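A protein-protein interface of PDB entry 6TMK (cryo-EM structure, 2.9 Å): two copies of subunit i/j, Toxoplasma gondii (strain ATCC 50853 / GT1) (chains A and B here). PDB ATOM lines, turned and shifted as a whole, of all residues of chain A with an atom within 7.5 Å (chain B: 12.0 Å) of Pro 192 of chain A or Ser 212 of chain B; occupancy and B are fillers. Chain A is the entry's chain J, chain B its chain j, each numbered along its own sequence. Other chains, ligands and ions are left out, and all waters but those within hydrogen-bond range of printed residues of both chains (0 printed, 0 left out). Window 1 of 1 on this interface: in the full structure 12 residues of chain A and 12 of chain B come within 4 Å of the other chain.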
ATOM      1  N   ARG A 178      14.486  -2.482   0.605  1.00  0.00           N
ATOM      2  CA  ARG A 178      13.924  -3.772   0.982  1.00  0.00           C
ATOM      3  C   ARG A 178      14.918  -4.905   0.769  1.00  0.00           C
ATOM      4  O   ARG A 178      15.020  -5.816   1.599  1.00  0.00           O
ATOM      5  CB  ARG A 178      12.651  -4.019   0.184  1.00  0.00           C
ATOM      6  CG  ARG A 178      11.910  -5.281   0.538  1.00  0.00           C
ATOM      7  CD  ARG A 178      10.677  -5.447  -0.304  1.00  0.00           C
ATOM      8  NE  ARG A 178      10.134  -6.794  -0.213  1.00  0.00           N
ATOM      9  CZ  ARG A 178      10.479  -7.801  -1.005  1.00  0.00           C
ATOM     10  NH1 ARG A 178      11.375  -7.638  -1.958  1.00  0.00           N
ATOM     11  NH2 ARG A 178       9.929  -8.981  -0.831  1.00  0.00           N
ATOM     12  N   LEU A 182      16.307  -7.491   3.614  1.00  0.00           N
ATOM     13  CA  LEU A 182      16.198  -8.940   3.520  1.00  0.00           C
ATOM     14  C   LEU A 182      17.562  -9.609   3.551  1.00  0.00           C
ATOM     15  O   LEU A 182      17.725 -10.670   4.162  1.00  0.00           O
ATOM     16  CB  LEU A 182      15.454  -9.323   2.249  1.00  0.00           C
ATOM     17  CG  LEU A 182      13.989  -8.936   2.175  1.00  0.00           C
ATOM     18  CD1 LEU A 182      13.442  -9.363   0.857  1.00  0.00           C
ATOM     19  CD2 LEU A 182      13.206  -9.569   3.298  1.00  0.00           C
ATOM     20  N   ILE A 189      20.141 -15.531   1.568  1.00  0.00           N
ATOM     21  CA  ILE A 189      19.047 -15.389   0.623  1.00  0.00           C
ATOM     22  C   ILE A 189      19.593 -15.084  -0.768  1.00  0.00           C
ATOM     23  O   ILE A 189      20.653 -14.471  -0.931  1.00  0.00           O
ATOM     24  CB  ILE A 189      18.083 -14.301   1.125  1.00  0.00           C
ATOM     25  CG1 ILE A 189      16.769 -14.318   0.353  1.00  0.00           C
ATOM     26  CG2 ILE A 189      18.739 -12.941   1.087  1.00  0.00           C
ATOM     27  CD1 ILE A 189      15.726 -13.484   0.984  1.00  0.00           C
ATOM     28  N   GLN A 190      18.852 -15.516  -1.782  1.00  0.00           N
ATOM     29  CA  GLN A 190      19.392 -15.627  -3.128  1.00  0.00           C
ATOM     30  C   GLN A 190      18.272 -15.274  -4.107  1.00  0.00           C
ATOM     31  O   GLN A 190      17.232 -14.737  -3.713  1.00  0.00           O
ATOM     32  CB  GLN A 190      20.017 -17.023  -3.263  1.00  0.00           C
ATOM     33  CG  GLN A 190      21.167 -17.079  -4.190  1.00  0.00           C
ATOM     34  CD  GLN A 190      22.151 -18.136  -3.807  1.00  0.00           C
ATOM     35  OE1 GLN A 190      22.179 -18.609  -2.676  1.00  0.00           O
ATOM     36  NE2 GLN A 190      23.008 -18.469  -4.724  1.00  0.00           N
ATOM     37  N   PHE A 191      18.442 -15.609  -5.392  1.00  0.00           N
ATOM     38  CA  PHE A 191      17.788 -14.920  -6.504  1.00  0.00           C
ATOM     39  C   PHE A 191      16.288 -14.720  -6.362  1.00  0.00           C
ATOM     40  O   PHE A 191      15.825 -13.572  -6.393  1.00  0.00           O
ATOM     41  CB  PHE A 191      18.022 -15.572  -7.863  1.00  0.00           C
ATOM     42  CG  PHE A 191      16.956 -15.218  -8.853  1.00  0.00           C
ATOM     43  CD1 PHE A 191      16.733 -13.913  -9.212  1.00  0.00           C
ATOM     44  CD2 PHE A 191      16.195 -16.201  -9.448  1.00  0.00           C
ATOM     45  CE1 PHE A 191      15.732 -13.590 -10.087  1.00  0.00           C
ATOM     46  CE2 PHE A 191      15.205 -15.877 -10.334  1.00  0.00           C
ATOM     47  CZ  PHE A 191      14.992 -14.572 -10.670  1.00  0.00           C
ATOM     48  N   PRO A 192      15.494 -15.774  -6.209  1.00  0.00           N
ATOM     49  CA  PRO A 192      14.047 -15.626  -6.411  1.00  0.00           C
ATOM     50  C   PRO A 192      13.441 -14.596  -5.489  1.00  0.00           C
ATOM     51  O   PRO A 192      12.392 -14.034  -5.814  1.00  0.00           O
ATOM     52  CB  PRO A 192      13.504 -17.040  -6.149  1.00  0.00           C
ATOM     53  CG  PRO A 192      14.669 -17.923  -6.251  1.00  0.00           C
ATOM     54  CD  PRO A 192      15.860 -17.145  -5.844  1.00  0.00           C
ATOM     55  N   PHE A 193      14.090 -14.298  -4.374  1.00  0.00           N
ATOM     56  CA  PHE A 193      13.618 -13.326  -3.407  1.00  0.00           C
ATOM     57  C   PHE A 193      14.400 -12.023  -3.457  1.00  0.00           C
ATOM     58  O   PHE A 193      13.835 -10.969  -3.174  1.00  0.00           O
ATOM     59  CB  PHE A 193      13.679 -13.919  -1.998  1.00  0.00           C
ATOM     60  CG  PHE A 193      13.047 -15.264  -1.892  1.00  0.00           C
ATOM     61  CD1 PHE A 193      11.677 -15.393  -1.869  1.00  0.00           C
ATOM     62  CD2 PHE A 193      13.817 -16.401  -1.818  1.00  0.00           C
ATOM     63  CE1 PHE A 193      11.095 -16.618  -1.778  1.00  0.00           C
ATOM     64  CE2 PHE A 193      13.232 -17.632  -1.724  1.00  0.00           C
ATOM     65  CZ  PHE A 193      11.873 -17.739  -1.700  1.00  0.00           C
ATOM     66  N   VAL A 194      15.675 -12.072  -3.832  1.00  0.00           N
ATOM     67  CA  VAL A 194      16.498 -10.888  -4.042  1.00  0.00           C
ATOM     68  C   VAL A 194      17.420 -11.161  -5.216  1.00  0.00           C
ATOM     69  O   VAL A 194      17.872 -12.287  -5.419  1.00  0.00           O
ATOM     70  CB  VAL A 194      17.351 -10.517  -2.809  1.00  0.00           C
ATOM     71  CG1 VAL A 194      16.514 -10.354  -1.587  1.00  0.00           C
ATOM     72  CG2 VAL A 194      18.398 -11.582  -2.576  1.00  0.00           C
ATOM     73  N   PHE A 195      17.706 -10.121  -5.994  1.00  0.00           N
ATOM     74  CA  PHE A 195      18.555 -10.277  -7.172  1.00  0.00           C
ATOM     75  C   PHE A 195      19.985 -10.504  -6.710  1.00  0.00           C
ATOM     76  O   PHE A 195      20.723  -9.559  -6.436  1.00  0.00           O
ATOM     77  CB  PHE A 195      18.466  -9.061  -8.082  1.00  0.00           C
ATOM     78  CG  PHE A 195      17.244  -9.036  -8.940  1.00  0.00           C
ATOM     79  CD1 PHE A 195      17.031  -9.999  -9.898  1.00  0.00           C
ATOM     80  CD2 PHE A 195      16.312  -8.037  -8.796  1.00  0.00           C
ATOM     81  CE1 PHE A 195      15.910  -9.971 -10.674  1.00  0.00           C
ATOM     82  CE2 PHE A 195      15.200  -8.007  -9.571  1.00  0.00           C
ATOM     83  CZ  PHE A 195      14.999  -8.972 -10.515  1.00  0.00           C
ATOM     84  N   ARG A 196      20.383 -11.766  -6.640  1.00  0.00           N
ATOM     85  CA  ARG A 196      21.682 -12.133  -6.110  1.00  0.00           C
ATOM     86  C   ARG A 196      21.914 -13.603  -6.398  1.00  0.00           C
ATOM     87  O   ARG A 196      21.003 -14.417  -6.246  1.00  0.00           O
ATOM     88  CB  ARG A 196      21.753 -11.855  -4.605  1.00  0.00           C
ATOM     89  CG  ARG A 196      23.015 -12.311  -3.937  1.00  0.00           C
ATOM     90  CD  ARG A 196      23.286 -11.606  -2.641  1.00  0.00           C
ATOM     91  NE  ARG A 196      22.767 -12.316  -1.486  1.00  0.00           N
ATOM     92  CZ  ARG A 196      23.203 -12.131  -0.247  1.00  0.00           C
ATOM     93  NH1 ARG A 196      24.163 -11.260  -0.001  1.00  0.00           N
ATOM     94  NH2 ARG A 196      22.673 -12.817   0.744  1.00  0.00           N
ATOM     95  N   GLN A 197      23.122 -13.925  -6.837  1.00  0.00           N
ATOM     96  CA  GLN A 197      23.512 -15.293  -7.137  1.00  0.00           C
ATOM     97  C   GLN A 197      24.931 -15.528  -6.652  1.00  0.00           C
ATOM     98  O   GLN A 197      25.829 -14.744  -6.960  1.00  0.00           O
ATOM     99  CB  GLN A 197      23.410 -15.586  -8.633  1.00  0.00           C
ATOM    100  CG  GLN A 197      22.040 -15.424  -9.223  1.00  0.00           C
ATOM    101  CD  GLN A 197      21.889 -14.185 -10.065  1.00  0.00           C
ATOM    102  OE1 GLN A 197      22.851 -13.675 -10.632  1.00  0.00           O
ATOM    103  NE2 GLN A 197      20.669 -13.688 -10.148  1.00  0.00           N
ATOM    104  N   GLU B 208      10.418 -11.903 -19.254  1.00  0.00           N
ATOM    105  CA  GLU B 208      10.641 -11.035 -18.112  1.00  0.00           C
ATOM    106  C   GLU B 208      11.102 -11.832 -16.903  1.00  0.00           C
ATOM    107  O   GLU B 208      10.680 -12.971 -16.694  1.00  0.00           O
ATOM    108  CB  GLU B 208       9.373 -10.259 -17.774  1.00  0.00           C
ATOM    109  CG  GLU B 208       9.060  -9.172 -18.770  1.00  0.00           C
ATOM    110  CD  GLU B 208      10.029  -8.008 -18.678  1.00  0.00           C
ATOM    111  OE1 GLU B 208      10.667  -7.682 -19.699  1.00  0.00           O
ATOM    112  OE2 GLU B 208      10.160  -7.424 -17.582  1.00  0.00           O
ATOM    113  N   VAL B 209      11.984 -11.224 -16.117  1.00  0.00           N
ATOM    114  CA  VAL B 209      12.567 -11.850 -14.939  1.00  0.00           C
ATOM    115  C   VAL B 209      12.283 -10.964 -13.738  1.00  0.00           C
ATOM    116  O   VAL B 209      12.716  -9.806 -13.697  1.00  0.00           O
ATOM    117  CB  VAL B 209      14.078 -12.083 -15.091  1.00  0.00           C
ATOM    118  CG1 VAL B 209      14.620 -12.734 -13.842  1.00  0.00           C
ATOM    119  CG2 VAL B 209      14.364 -12.936 -16.287  1.00  0.00           C
ATOM    120  N   HIS B 210      11.560 -11.504 -12.766  1.00  0.00           N
ATOM    121  CA  HIS B 210      11.201 -10.778 -11.565  1.00  0.00           C
ATOM    122  C   HIS B 210      11.551 -11.615 -10.350  1.00  0.00           C
ATOM    123  O   HIS B 210      11.742 -12.829 -10.440  1.00  0.00           O
ATOM    124  CB  HIS B 210       9.712 -10.431 -11.529  1.00  0.00           C
ATOM    125  CG  HIS B 210       9.260  -9.586 -12.672  1.00  0.00           C
ATOM    126  ND1 HIS B 210       9.732  -8.309 -12.881  1.00  0.00           N
ATOM    127  CD2 HIS B 210       8.389  -9.836 -13.674  1.00  0.00           C
ATOM    128  CE1 HIS B 210       9.164  -7.807 -13.962  1.00  0.00           C
ATOM    129  NE2 HIS B 210       8.344  -8.713 -14.460  1.00  0.00           N
ATOM    130  N   THR B 211      11.636 -10.949  -9.207  1.00  0.00           N
ATOM    131  CA  THR B 211      11.845 -11.646  -7.954  1.00  0.00           C
ATOM    132  C   THR B 211      10.526 -12.250  -7.504  1.00  0.00           C
ATOM    133  O   THR B 211       9.465 -11.643  -7.657  1.00  0.00           O
ATOM    134  CB  THR B 211      12.394 -10.702  -6.888  1.00  0.00           C
ATOM    135  OG1 THR B 211      11.619  -9.502  -6.853  1.00  0.00           O
ATOM    136  CG2 THR B 211      13.824 -10.361  -7.192  1.00  0.00           C
ATOM    137  N   SER B 212      10.599 -13.456  -6.958  1.00  0.00           N
ATOM    138  CA  SER B 212       9.450 -14.046  -6.300  1.00  0.00           C
ATOM    139  C   SER B 212       8.982 -13.149  -5.158  1.00  0.00           C
ATOM    140  O   SER B 212       9.780 -12.418  -4.567  1.00  0.00           O
ATOM    141  CB  SER B 212       9.778 -15.436  -5.773  1.00  0.00           C
ATOM    142  OG  SER B 212      10.077 -16.315  -6.833  1.00  0.00           O
ATOM    143  N   PRO B 213       7.698 -13.185  -4.821  1.00  0.00           N
ATOM    144  CA  PRO B 213       7.266 -12.555  -3.574  1.00  0.00           C
ATOM    145  C   PRO B 213       7.786 -13.306  -2.365  1.00  0.00           C
ATOM    146  O   PRO B 213       8.039 -14.512  -2.408  1.00  0.00           O
ATOM    147  CB  PRO B 213       5.737 -12.630  -3.650  1.00  0.00           C
ATOM    148  CG  PRO B 213       5.453 -13.670  -4.649  1.00  0.00           C
ATOM    149  CD  PRO B 213       6.555 -13.641  -5.623  1.00  0.00           C
ATOM    150  N   ALA B 214       7.941 -12.569  -1.273  1.00  0.00           N
ATOM    151  CA  ALA B 214       8.336 -13.178  -0.015  1.00  0.00           C
ATOM    152  C   ALA B 214       7.284 -14.173   0.455  1.00  0.00           C
ATOM    153  O   ALA B 214       6.095 -14.045   0.157  1.00  0.00           O
ATOM    154  CB  ALA B 214       8.555 -12.100   1.043  1.00  0.00           C
ATOM    155  N   LEU B 215       7.737 -15.180   1.194  1.00  0.00           N
ATOM    156  CA  LEU B 215       6.835 -16.214   1.671  1.00  0.00           C
ATOM    157  C   LEU B 215       5.770 -15.618   2.580  1.00  0.00           C
ATOM    158  O   LEU B 215       6.034 -14.700   3.361  1.00  0.00           O
ATOM    159  CB  LEU B 215       7.618 -17.297   2.403  1.00  0.00           C
ATOM    160  CG  LEU B 215       8.713 -17.962   1.569  1.00  0.00           C
ATOM    161  CD1 LEU B 215       9.449 -18.975   2.391  1.00  0.00           C
ATOM    162  CD2 LEU B 215       8.142 -18.625   0.326  1.00  0.00           C
ATOM    163  N   GLN B 216       4.559 -16.150   2.469  1.00  0.00           N
ATOM    164  CA  GLN B 216       3.413 -15.565   3.145  1.00  0.00           C
ATOM    165  C   GLN B 216       3.585 -15.644   4.654  1.00  0.00           C
ATOM    166  O   GLN B 216       3.817 -16.720   5.211  1.00  0.00           O
ATOM    167  CB  GLN B 216       2.134 -16.271   2.712  1.00  0.00           C
ATOM    168  CG  GLN B 216       1.689 -15.919   1.314  1.00  0.00           C
ATOM    169  CD  GLN B 216       0.944 -14.606   1.247  1.00  0.00           C
ATOM    170  OE1 GLN B 216       1.399 -13.646   0.625  1.00  0.00           O
ATOM    171  NE2 GLN B 216      -0.210 -14.560   1.880  1.00  0.00           N
ATOM    172  N   GLN B 217       3.480 -14.492   5.312  1.00  0.00           N
ATOM    173  CA  GLN B 217       3.463 -14.437   6.766  1.00  0.00           C
ATOM    174  C   GLN B 217       2.257 -15.165   7.341  1.00  0.00           C
ATOM    175  O   GLN B 217       1.116 -14.726   7.169  1.00  0.00           O
ATOM    176  CB  GLN B 217       3.450 -12.987   7.244  1.00  0.00           C
ATOM    177  CG  GLN B 217       4.762 -12.253   7.090  1.00  0.00           C
ATOM    178  CD  GLN B 217       4.741 -10.903   7.777  1.00  0.00           C
ATOM    179  OE1 GLN B 217       4.962  -9.870   7.148  1.00  0.00           O
ATOM    180  NE2 GLN B 217       4.462 -10.905   9.076  1.00  0.00           N
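OG of Ser 212 of chain B lies close to O of Pro 192 of chain A, 3.4 Å away.
N of Phe 191 of chain A sits at hydrogen-bond distance from O of Arg 196 of chain A.
NH2 of Arg 178 of chain A touches CB of Ala 214 of chain B (3.9 Å). Val 209 of chain B touches Phe 191 of chain A. O of His 210 of chain B touches CZ of Phe 191 of chain A, at 3.7 Å. O of Phe 191 of chain A touches CG2 of Thr 211 of chain B (3.9 Å). O of Pro 192 of chain A touches C of Thr 211 of chain B (3.1 Å). CB of Thr 211 of chain B touches O of Phe 193 of chain A, at 3.99 Å. Phe 193 of chain A touches Pro 213 of chain B (CE1 to O, 3.8 Å). Thr 211 of chain B touches Phe 195 of chain A.
Printed residues of chain B within 4 Å of Arg 178 of chain A: Ala 214 (3.9 Å). No residue of chain B comes within 4 Å of Gln 190 of chain A. Of chain B, only Val 209, His 210 and Thr 211 come within 4 Å of Phe 191 of chain A. Pro 192 of chain A touches two residues of chain B. No residue of chain B comes within 4 Å of Val 194 of chain A. Of the printed residues of chain A, Val 209 of chain B touches Phe 191 (3.7 Å). Ser 212 of chain B touches just one residue of chain A: Pro 192 (2.2 Å). Printed residues of chain A within 4 Å of Pro 213 of chain B: Phe 193 (3.8 Å). The nearest residue of chain B that does not touch Pro 192 of chain A is His 210 of chain B (4.8 Å). The nearest residue of chain A that does not touch Ser 212 of chain B is Phe 193 of chain A (4.1 Å). The nearest printed residue of chain B that does not touch Phe 195 of chain A is Val 209 of chain B (4.004 Å).
Of the 11 printed residues of chain A, 5 touch a printed residue of chain B. Hydrophobic or aromatic side chains of chain A within 4 Å of the printed part of chain B: Phe 191, Pro 192, Phe 193 and Phe 195. Among the printed residues, 9 pairs touch across the chains.
No position is printed for both chains.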
